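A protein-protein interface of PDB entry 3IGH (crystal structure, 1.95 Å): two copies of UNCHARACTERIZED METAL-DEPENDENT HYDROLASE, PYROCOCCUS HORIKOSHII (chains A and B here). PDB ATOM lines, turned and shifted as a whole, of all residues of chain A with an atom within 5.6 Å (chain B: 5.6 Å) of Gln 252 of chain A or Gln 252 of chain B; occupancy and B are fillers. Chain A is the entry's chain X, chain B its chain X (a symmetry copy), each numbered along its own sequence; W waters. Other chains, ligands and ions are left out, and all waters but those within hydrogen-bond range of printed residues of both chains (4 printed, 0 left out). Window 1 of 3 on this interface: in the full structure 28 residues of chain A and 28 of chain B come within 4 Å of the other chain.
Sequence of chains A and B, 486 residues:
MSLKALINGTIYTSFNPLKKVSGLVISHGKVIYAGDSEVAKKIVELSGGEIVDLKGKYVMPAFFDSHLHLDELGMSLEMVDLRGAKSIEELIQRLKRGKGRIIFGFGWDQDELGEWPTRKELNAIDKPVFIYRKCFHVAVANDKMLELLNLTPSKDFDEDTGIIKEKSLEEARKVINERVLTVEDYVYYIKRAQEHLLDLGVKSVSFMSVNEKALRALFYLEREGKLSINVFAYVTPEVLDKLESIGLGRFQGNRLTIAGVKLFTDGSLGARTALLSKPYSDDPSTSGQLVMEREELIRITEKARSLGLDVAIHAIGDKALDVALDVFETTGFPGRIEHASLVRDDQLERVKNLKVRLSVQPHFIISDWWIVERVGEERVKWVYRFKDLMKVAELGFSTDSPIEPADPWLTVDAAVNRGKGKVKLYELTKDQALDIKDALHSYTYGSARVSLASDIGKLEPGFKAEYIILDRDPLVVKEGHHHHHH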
ATOM      1  N   GLU A 222      -7.664  -2.826  -9.185  1.00  0.00           N
ATOM      2  CA  GLU A 222      -8.873  -3.046  -8.377  1.00  0.00           C
ATOM      3  C   GLU A 222      -9.551  -1.732  -7.935  1.00  0.00           C
ATOM      4  O   GLU A 222     -10.759  -1.586  -8.124  1.00  0.00           O
ATOM      5  CB  GLU A 222      -8.569  -3.983  -7.188  1.00  0.00           C
ATOM      6  CG  GLU A 222      -9.592  -4.009  -6.034  1.00  0.00           C
ATOM      7  CD  GLU A 222     -10.820  -4.887  -6.278  1.00  0.00           C
ATOM      8  OE1 GLU A 222     -10.881  -5.623  -7.288  1.00  0.00           O
ATOM      9  OE2 GLU A 222     -11.737  -4.838  -5.430  1.00  0.00           O
ATOM     10  N   PHE A 232      -7.367 -14.385  -8.293  1.00  0.00           N
ATOM     11  CA  PHE A 232      -7.058 -14.956  -6.988  1.00  0.00           C
ATOM     12  C   PHE A 232      -5.530 -14.959  -6.830  1.00  0.00           C
ATOM     13  O   PHE A 232      -4.829 -15.800  -7.407  1.00  0.00           O
ATOM     14  CB  PHE A 232      -7.700 -16.351  -6.845  1.00  0.00           C
ATOM     15  CG  PHE A 232      -9.210 -16.305  -6.800  1.00  0.00           C
ATOM     16  CD1 PHE A 232      -9.881 -16.346  -5.576  1.00  0.00           C
ATOM     17  CD2 PHE A 232      -9.961 -16.149  -7.976  1.00  0.00           C
ATOM     18  CE1 PHE A 232     -11.274 -16.253  -5.519  1.00  0.00           C
ATOM     19  CE2 PHE A 232     -11.359 -16.062  -7.934  1.00  0.00           C
ATOM     20  CZ  PHE A 232     -12.014 -16.110  -6.698  1.00  0.00           C
ATOM     21  N   ARG A 250      -6.784 -13.530   3.984  1.00  0.00           N
ATOM     22  CA  ARG A 250      -7.743 -13.644   2.882  1.00  0.00           C
ATOM     23  C   ARG A 250      -8.660 -12.428   2.885  1.00  0.00           C
ATOM     24  O   ARG A 250      -9.174 -12.016   3.935  1.00  0.00           O
ATOM     25  CB  ARG A 250      -8.545 -14.955   2.891  1.00  0.00           C
ATOM     26  CG  ARG A 250      -9.284 -15.180   1.556  1.00  0.00           C
ATOM     27  CD  ARG A 250      -9.709 -16.614   1.304  1.00  0.00           C
ATOM     28  NE  ARG A 250      -9.986 -16.858  -0.117  1.00  0.00           N
ATOM     29  CZ  ARG A 250      -9.263 -17.655  -0.905  1.00  0.00           C
ATOM     30  NH1 ARG A 250      -8.213 -18.309  -0.419  1.00  0.00           N
ATOM     31  NH2 ARG A 250      -9.596 -17.812  -2.186  1.00  0.00           N
ATOM     32  N   PHE A 251      -8.821 -11.840   1.704  1.00  0.00           N
ATOM     33  CA  PHE A 251      -9.600 -10.623   1.536  1.00  0.00           C
ATOM     34  C   PHE A 251     -10.188 -10.648   0.128  1.00  0.00           C
ATOM     35  O   PHE A 251      -9.440 -10.672  -0.860  1.00  0.00           O
ATOM     36  CB  PHE A 251      -8.679  -9.404   1.728  1.00  0.00           C
ATOM     37  CG  PHE A 251      -9.387  -8.123   2.141  1.00  0.00           C
ATOM     38  CD1 PHE A 251     -10.651  -8.136   2.717  1.00  0.00           C
ATOM     39  CD2 PHE A 251      -8.744  -6.889   1.984  1.00  0.00           C
ATOM     40  CE1 PHE A 251     -11.278  -6.936   3.097  1.00  0.00           C
ATOM     41  CE2 PHE A 251      -9.353  -5.689   2.372  1.00  0.00           C
ATOM     42  CZ  PHE A 251     -10.626  -5.714   2.928  1.00  0.00           C
ATOM     43  N   GLN A 252     -11.511 -10.644   0.053  1.00  0.00           N
ATOM     44  CA  GLN A 252     -12.196 -10.722  -1.219  1.00  0.00           C
ATOM     45  C   GLN A 252     -12.774  -9.355  -1.571  1.00  0.00           C
ATOM     46  O   GLN A 252     -13.681  -8.847  -0.902  1.00  0.00           O
ATOM     47  CB  GLN A 252     -13.273 -11.804  -1.150  1.00  0.00           C
ATOM     48  CG  GLN A 252     -13.371 -12.661  -2.392  1.00  0.00           C
ATOM     49  CD  GLN A 252     -14.662 -12.455  -3.139  1.00  0.00           C
ATOM     50  OE1 GLN A 252     -15.740 -12.730  -2.615  1.00  0.00           O
ATOM     51  NE2 GLN A 252     -14.565 -11.983  -4.377  1.00  0.00           N
ATOM     52  N   GLY A 253     -12.211  -8.748  -2.609  1.00  0.00           N
ATOM     53  CA  GLY A 253     -12.695  -7.476  -3.129  1.00  0.00           C
ATOM     54  C   GLY A 253     -13.686  -7.714  -4.244  1.00  0.00           C
ATOM     55  O   GLY A 253     -14.340  -8.761  -4.299  1.00  0.00           O
ATOM     56  N   ASN A 254     -13.792  -6.741  -5.139  1.00  0.00           N
ATOM     57  CA  ASN A 254     -14.698  -6.828  -6.269  1.00  0.00           C
ATOM     58  C   ASN A 254     -14.198  -7.833  -7.313  1.00  0.00           C
ATOM     59  O   ASN A 254     -14.908  -8.750  -7.701  1.00  0.00           O
ATOM     60  CB  ASN A 254     -14.850  -5.444  -6.897  1.00  0.00           C
ATOM     61  CG  ASN A 254     -15.777  -5.444  -8.086  1.00  0.00           C
ATOM     62  OD1 ASN A 254     -16.845  -6.063  -8.062  1.00  0.00           O
ATOM     63  ND2 ASN A 254     -15.373  -4.751  -9.139  1.00  0.00           N
ATOM     64  N   LEU A 256     -10.419  -8.567  -7.227  1.00  0.00           N
ATOM     65  CA  LEU A 256      -9.192  -9.073  -6.622  1.00  0.00           C
ATOM     66  C   LEU A 256      -9.466  -9.773  -5.295  1.00  0.00           C
ATOM     67  O   LEU A 256     -10.132  -9.220  -4.408  1.00  0.00           O
ATOM     68  CB  LEU A 256      -8.196  -7.920  -6.407  1.00  0.00           C
ATOM     69  CG  LEU A 256      -6.852  -8.239  -5.728  1.00  0.00           C
ATOM     70  CD1 LEU A 256      -6.004  -9.176  -6.616  1.00  0.00           C
ATOM     71  CD2 LEU A 256      -6.089  -6.951  -5.401  1.00  0.00           C
ATOM     72  N   THR A 257      -8.939 -10.987  -5.169  1.00  0.00           N
ATOM     73  CA  THR A 257      -8.899 -11.709  -3.906  1.00  0.00           C
ATOM     74  C   THR A 257      -7.443 -11.908  -3.498  1.00  0.00           C
ATOM     75  O   THR A 257      -6.639 -12.439  -4.279  1.00  0.00           O
ATOM     76  CB  THR A 257      -9.548 -13.108  -4.041  1.00  0.00           C
ATOM     77  OG1 THR A 257     -10.854 -12.968  -4.609  1.00  0.00           O
ATOM     78  CG2 THR A 257      -9.655 -13.822  -2.681  1.00  0.00           C
ATOM     79  N   ILE A 258      -7.097 -11.489  -2.283  1.00  0.00           N
ATOM     80  CA  ILE A 258      -5.827 -11.907  -1.682  1.00  0.00           C
ATOM     81  C   ILE A 258      -6.105 -13.330  -1.222  1.00  0.00           C
ATOM     82  O   ILE A 258      -6.850 -13.537  -0.266  1.00  0.00           O
ATOM     83  CB  ILE A 258      -5.412 -10.984  -0.499  1.00  0.00           C
ATOM     84  CG1 ILE A 258      -5.443  -9.509  -0.927  1.00  0.00           C
ATOM     85  CG2 ILE A 258      -4.028 -11.386   0.064  1.00  0.00           C
ATOM     86  CD1 ILE A 258      -4.588  -9.171  -2.170  1.00  0.00           C
ATOM     87  N   ASP A 455     -18.252 -19.180  -5.187  1.00  0.00           N
ATOM     88  CA  ASP A 455     -19.357 -18.671  -6.005  1.00  0.00           C
ATOM     89  C   ASP A 455     -19.015 -18.548  -7.495  1.00  0.00           C
ATOM     90  O   ASP A 455     -19.632 -17.774  -8.214  1.00  0.00           O
ATOM     91  CB  ASP A 455     -19.881 -17.344  -5.442  1.00  0.00           C
ATOM     92  CG  ASP A 455     -18.803 -16.269  -5.360  1.00  0.00           C
ATOM     93  OD1 ASP A 455     -17.625 -16.559  -5.664  1.00  0.00           O
ATOM     94  OD2 ASP A 455     -19.135 -15.125  -4.987  1.00  0.00           O
ATOM     95  N   LYS A 464     -21.603 -16.323  -9.366  1.00  0.00           N
ATOM     96  CA  LYS A 464     -21.301 -15.179 -10.226  1.00  0.00           C
ATOM     97  C   LYS A 464     -21.648 -15.522 -11.678  1.00  0.00           C
ATOM     98  O   LYS A 464     -21.400 -16.641 -12.136  1.00  0.00           O
ATOM     99  CB  LYS A 464     -19.824 -14.776 -10.137  1.00  0.00           C
ATOM    100  CG  LYS A 464     -19.413 -14.149  -8.809  1.00  0.00           C
ATOM    101  CD  LYS A 464     -18.051 -13.462  -8.917  1.00  0.00           C
ATOM    102  CE  LYS A 464     -17.704 -12.749  -7.618  1.00  0.00           C
ATOM    103  NZ  LYS A 464     -16.555 -11.807  -7.763  1.00  0.00           N
ATOM    104  N   GLU B 222     -13.392  -9.749   9.435  1.00  0.00           N
ATOM    105  CA  GLU B 222     -13.790  -9.829   8.022  1.00  0.00           C
ATOM    106  C   GLU B 222     -13.565 -11.228   7.409  1.00  0.00           C
ATOM    107  O   GLU B 222     -14.485 -11.770   6.796  1.00  0.00           O
ATOM    108  CB  GLU B 222     -13.112  -8.709   7.203  1.00  0.00           C
ATOM    109  CG  GLU B 222     -13.097  -8.871   5.669  1.00  0.00           C
ATOM    110  CD  GLU B 222     -14.390  -8.463   4.963  1.00  0.00           C
ATOM    111  OE1 GLU B 222     -15.313  -7.910   5.602  1.00  0.00           O
ATOM    112  OE2 GLU B 222     -14.474  -8.699   3.738  1.00  0.00           O
ATOM    113  N   PHE B 232     -16.275   1.328   7.568  1.00  0.00           N
ATOM    114  CA  PHE B 232     -15.404   2.118   6.709  1.00  0.00           C
ATOM    115  C   PHE B 232     -14.235   2.624   7.567  1.00  0.00           C
ATOM    116  O   PHE B 232     -14.381   3.569   8.354  1.00  0.00           O
ATOM    117  CB  PHE B 232     -16.203   3.245   6.022  1.00  0.00           C
ATOM    118  CG  PHE B 232     -17.215   2.729   5.026  1.00  0.00           C
ATOM    119  CD1 PHE B 232     -16.914   2.701   3.663  1.00  0.00           C
ATOM    120  CD2 PHE B 232     -18.445   2.204   5.456  1.00  0.00           C
ATOM    121  CE1 PHE B 232     -17.822   2.179   2.739  1.00  0.00           C
ATOM    122  CE2 PHE B 232     -19.369   1.684   4.539  1.00  0.00           C
ATOM    123  CZ  PHE B 232     -19.050   1.669   3.176  1.00  0.00           C
ATOM    124  N   ARG B 250      -7.731   2.174  -1.268  1.00  0.00           N
ATOM    125  CA  ARG B 250      -9.144   1.846  -1.060  1.00  0.00           C
ATOM    126  C   ARG B 250      -9.398   0.412  -1.505  1.00  0.00           C
ATOM    127  O   ARG B 250      -8.955  -0.014  -2.581  1.00  0.00           O
ATOM    128  CB  ARG B 250     -10.115   2.826  -1.737  1.00  0.00           C
ATOM    129  CG  ARG B 250     -11.558   2.645  -1.225  1.00  0.00           C
ATOM    130  CD  ARG B 250     -12.471   3.829  -1.477  1.00  0.00           C
ATOM    131  NE  ARG B 250     -13.653   3.801  -0.606  1.00  0.00           N
ATOM    132  CZ  ARG B 250     -13.904   4.686   0.360  1.00  0.00           C
ATOM    133  NH1 ARG B 250     -13.065   5.693   0.586  1.00  0.00           N
ATOM    134  NH2 ARG B 250     -15.007   4.575   1.099  1.00  0.00           N
ATOM    135  N   PHE B 251     -10.082  -0.334  -0.642  1.00  0.00           N
ATOM    136  CA  PHE B 251     -10.349  -1.746  -0.868  1.00  0.00           C
ATOM    137  C   PHE B 251     -11.669  -2.076  -0.180  1.00  0.00           C
ATOM    138  O   PHE B 251     -11.787  -1.935   1.046  1.00  0.00           O
ATOM    139  CB  PHE B 251      -9.195  -2.578  -0.278  1.00  0.00           C
ATOM    140  CG  PHE B 251      -9.020  -3.959  -0.892  1.00  0.00           C
ATOM    141  CD1 PHE B 251      -9.539  -4.278  -2.140  1.00  0.00           C
ATOM    142  CD2 PHE B 251      -8.279  -4.935  -0.214  1.00  0.00           C
ATOM    143  CE1 PHE B 251      -9.354  -5.561  -2.687  1.00  0.00           C
ATOM    144  CE2 PHE B 251      -8.078  -6.211  -0.755  1.00  0.00           C
ATOM    145  CZ  PHE B 251      -8.619  -6.524  -1.995  1.00  0.00           C
ATOM    146  N   GLN B 252     -12.643  -2.508  -0.970  1.00  0.00           N
ATOM    147  CA  GLN B 252     -13.960  -2.804  -0.453  1.00  0.00           C
ATOM    148  C   GLN B 252     -14.158  -4.315  -0.393  1.00  0.00           C
ATOM    149  O   GLN B 252     -14.203  -5.001  -1.421  1.00  0.00           O
ATOM    150  CB  GLN B 252     -15.013  -2.120  -1.325  1.00  0.00           C
ATOM    151  CG  GLN B 252     -16.149  -1.492  -0.547  1.00  0.00           C
ATOM    152  CD  GLN B 252     -17.465  -2.184  -0.784  1.00  0.00           C
ATOM    153  OE1 GLN B 252     -17.970  -2.204  -1.904  1.00  0.00           O
ATOM    154  NE2 GLN B 252     -18.040  -2.745   0.274  1.00  0.00           N
ATOM    155  N   GLY B 253     -14.236  -4.832   0.828  1.00  0.00           N
ATOM    156  CA  GLY B 253     -14.505  -6.245   1.063  1.00  0.00           C
ATOM    157  C   GLY B 253     -15.988  -6.467   1.246  1.00  0.00           C
ATOM    158  O   GLY B 253     -16.812  -5.696   0.744  1.00  0.00           O
ATOM    159  N   ASN B 254     -16.327  -7.524   1.973  1.00  0.00           N
ATOM    160  CA  ASN B 254     -17.713  -7.864   2.239  1.00  0.00           C
ATOM    161  C   ASN B 254     -18.350  -6.885   3.232  1.00  0.00           C
ATOM    162  O   ASN B 254     -19.386  -6.293   2.962  1.00  0.00           O
ATOM    163  CB  ASN B 254     -17.783  -9.289   2.784  1.00  0.00           C
ATOM    164  CG  ASN B 254     -19.193  -9.725   3.091  1.00  0.00           C
ATOM    165  OD1 ASN B 254     -20.120  -9.477   2.315  1.00  0.00           O
ATOM    166  ND2 ASN B 254     -19.365 -10.375   4.232  1.00  0.00           N
ATOM    167  N   LEU B 256     -15.884  -4.987   5.499  1.00  0.00           N
ATOM    168  CA  LEU B 256     -14.799  -4.049   5.766  1.00  0.00           C
ATOM    169  C   LEU B 256     -14.362  -3.319   4.501  1.00  0.00           C
ATOM    170  O   LEU B 256     -14.084  -3.945   3.468  1.00  0.00           O
ATOM    171  CB  LEU B 256     -13.599  -4.792   6.379  1.00  0.00           C
ATOM    172  CG  LEU B 256     -12.325  -3.986   6.687  1.00  0.00           C
ATOM    173  CD1 LEU B 256     -12.598  -2.942   7.792  1.00  0.00           C
ATOM    174  CD2 LEU B 256     -11.174  -4.917   7.081  1.00  0.00           C
ATOM    175  N   THR B 257     -14.297  -1.995   4.597  1.00  0.00           N
ATOM    176  CA  THR B 257     -13.689  -1.152   3.579  1.00  0.00           C
ATOM    177  C   THR B 257     -12.472  -0.454   4.179  1.00  0.00           C
ATOM    178  O   THR B 257     -12.578   0.206   5.223  1.00  0.00           O
ATOM    179  CB  THR B 257     -14.672  -0.057   3.099  1.00  0.00           C
ATOM    180  OG1 THR B 257     -15.905  -0.670   2.710  1.00  0.00           O
ATOM    181  CG2 THR B 257     -14.102   0.743   1.914  1.00  0.00           C
ATOM    182  N   ILE B 258     -11.318  -0.594   3.529  1.00  0.00           N
ATOM    183  CA  ILE B 258     -10.178   0.274   3.837  1.00  0.00           C
ATOM    184  C   ILE B 258     -10.528   1.579   3.140  1.00  0.00           C
ATOM    185  O   ILE B 258     -10.503   1.652   1.912  1.00  0.00           O
ATOM    186  CB  ILE B 258      -8.837  -0.322   3.315  1.00  0.00           C
ATOM    187  CG1 ILE B 258      -8.666  -1.772   3.796  1.00  0.00           C
ATOM    188  CG2 ILE B 258      -7.636   0.562   3.727  1.00  0.00           C
ATOM    189  CD1 ILE B 258      -8.757  -1.967   5.327  1.00  0.00           C
ATOM    190  N   ASP B 455     -23.418   2.762  -2.333  1.00  0.00           N
ATOM    191  CA  ASP B 455     -24.554   1.836  -2.360  1.00  0.00           C
ATOM    192  C   ASP B 455     -25.230   1.650  -0.996  1.00  0.00           C
ATOM    193  O   ASP B 455     -25.878   0.640  -0.753  1.00  0.00           O
ATOM    194  CB  ASP B 455     -24.139   0.488  -2.964  1.00  0.00           C
ATOM    195  CG  ASP B 455     -22.992  -0.173  -2.207  1.00  0.00           C
ATOM    196  OD1 ASP B 455     -22.455   0.437  -1.256  1.00  0.00           O
ATOM    197  OD2 ASP B 455     -22.623  -1.309  -2.566  1.00  0.00           O
ATOM    198  N   LYS B 464     -27.534  -1.487  -0.968  1.00  0.00           N
ATOM    199  CA  LYS B 464     -27.511  -2.570   0.013  1.00  0.00           C
ATOM    200  C   LYS B 464     -28.792  -2.531   0.851  1.00  0.00           C
ATOM    201  O   LYS B 464     -29.267  -1.454   1.224  1.00  0.00           O
ATOM    202  CB  LYS B 464     -26.293  -2.471   0.940  1.00  0.00           C
ATOM    203  CG  LYS B 464     -24.956  -2.772   0.271  1.00  0.00           C
ATOM    204  CD  LYS B 464     -23.855  -3.000   1.308  1.00  0.00           C
ATOM    205  CE  LYS B 464     -22.555  -3.406   0.630  1.00  0.00           C
ATOM    206  NZ  LYS B 464     -21.545  -3.945   1.588  1.00  0.00           N
HETATM  207  O   HOH W   1     -12.318  -2.861  -3.824  1.00  0.00           O
HETATM  208  O   HOH W   2     -16.200  -5.937  -2.937  1.00  0.00           O
HETATM  209  O   HOH W   3     -16.346  -8.780  -1.144  1.00  0.00           O
HETATM  210  O   HOH W   4     -13.224 -10.551   2.383  1.00  0.00           O
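The backbone NH of Asn 254 of chain A is in hydrogen-bond range of the side-chain carboxylate of Glu 222 of chain A (2.8 Å).
The backbone carbonyl oxygen (O) of Phe 251 of chain B lies within hydrogen-bond range of the backbone NH (N) of Ile 258 of chain B (2.9 Å).
The side-chain carboxylate (OE1) of Glu 222 of chain A sits at hydrogen-bond distance from the backbone NH (N) of Leu 256 of chain A (3.0 Å).
The side-chain carboxylate (OE2) of Glu 222 of chain B is in hydrogen-bond range of the backbone NH (N) of Asn 254 of chain B.
The backbone NH (N) of Leu 256 of chain B lies within hydrogen-bond range of the side-chain carboxylate (OE1) of Glu 222 of chain B (3.0 Å).
N of Ile 258 of chain A is in hydrogen-bond range of O of Phe 251 of chain A, 2.9 Å away.
Phe 251 of chain B touches Glu 222 of chain A.
Phe 251 of chain A touches Glu 222 of chain B.
Phe 251 of chain B touches Phe 251 of chain A (CE2 to CD2, 2.9 Å).
Phe 251 of chain A touches Gly 253 of chain B (CE1 to CA, 3.9 Å).
O of Leu 256 of chain B touches CZ of Phe 251 of chain A (3.9 Å).
Gln 252 of chain A touches Gln 252 of chain B.
Gly 253 of chain B touches Gln 252 of chain A.
Phe 251 of chain B touches Gly 253 of chain A (CE1 to CA, 3.9 Å).
Gly 253 of chain A touches Gln 252 of chain B.
Leu 256 of chain A touches Phe 251 of chain B.
Printed residues of chain B within 4 Å of Gln 252 of chain A: Gln 252 (3.9 Å) and Gly 253 (3.4 Å).
Thr 257 of chain A touches none of the printed residues of chain B.
Of the printed residues of chain A, Phe 251 of chain B touches Glu 222, Phe 251, Gly 253 and Leu 256.
Of the printed residues of chain A, Gln 252 of chain B touches Gln 252 and Gly 253.
Printed residues of chain A within 4 Å of Gly 253 of chain B: Phe 251 (3.9 Å) and Gln 252 (3.4 Å).
Of the printed residues of chain A, Leu 256 of chain B touches Phe 251 (3.9 Å).
Hydrophobic or aromatic side chains of chain B within 4 Å of the printed part of chain A: Phe 251.
Of the 12 printed residues of chain A, 5 touch a printed residue of chain B.
Hydrophobic or aromatic side chains of chain A within 4 Å of the printed part of chain B: Phe 251.
Along chain A the printed residues that touch a printed residue of chain B span positions 222 to 256.
Among the printed residues, no Asp or Glu carboxylate lies within 4 Å of a Lys or Arg side-chain nitrogen of the other chain.
Glu 222 of chain A touches Phe 251 of chain B, and with the chains exchanged Phe 251 of chain A touches Glu 222 of chain B.
Phe 251 of chain A touches Gly 253 of chain B, and with the chains exchanged Gly 253 of chain A touches Phe 251 of chain B.
Phe 251 of chain A touches Leu 256 of chain B, and with the chains exchanged Leu 256 of chain A touches Phe 251 of chain B.
Gln 252 of chain B touches its own counterpart, Gln 252 of chain A.
Of the 10 pairs that touch across the chains among the printed residues, 10 have their exchanged pair printed and touching as well.
Water W1 bridges OE2 of Glu 222 of chain A (2.6 Å) and N of Gln 252 of chain B (2.9 Å).
Water W4 bridges OE2 of Glu 222 of chain B and N of Gln 252 of chain A.
Water W3 bridges O of Gln 252 of chain A (2.7 Å) and N of Asn 254 of chain B (3.4 Å).
Water W2 bridges O of Gln 252 of chain B and N of Asn 254 of chain A.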
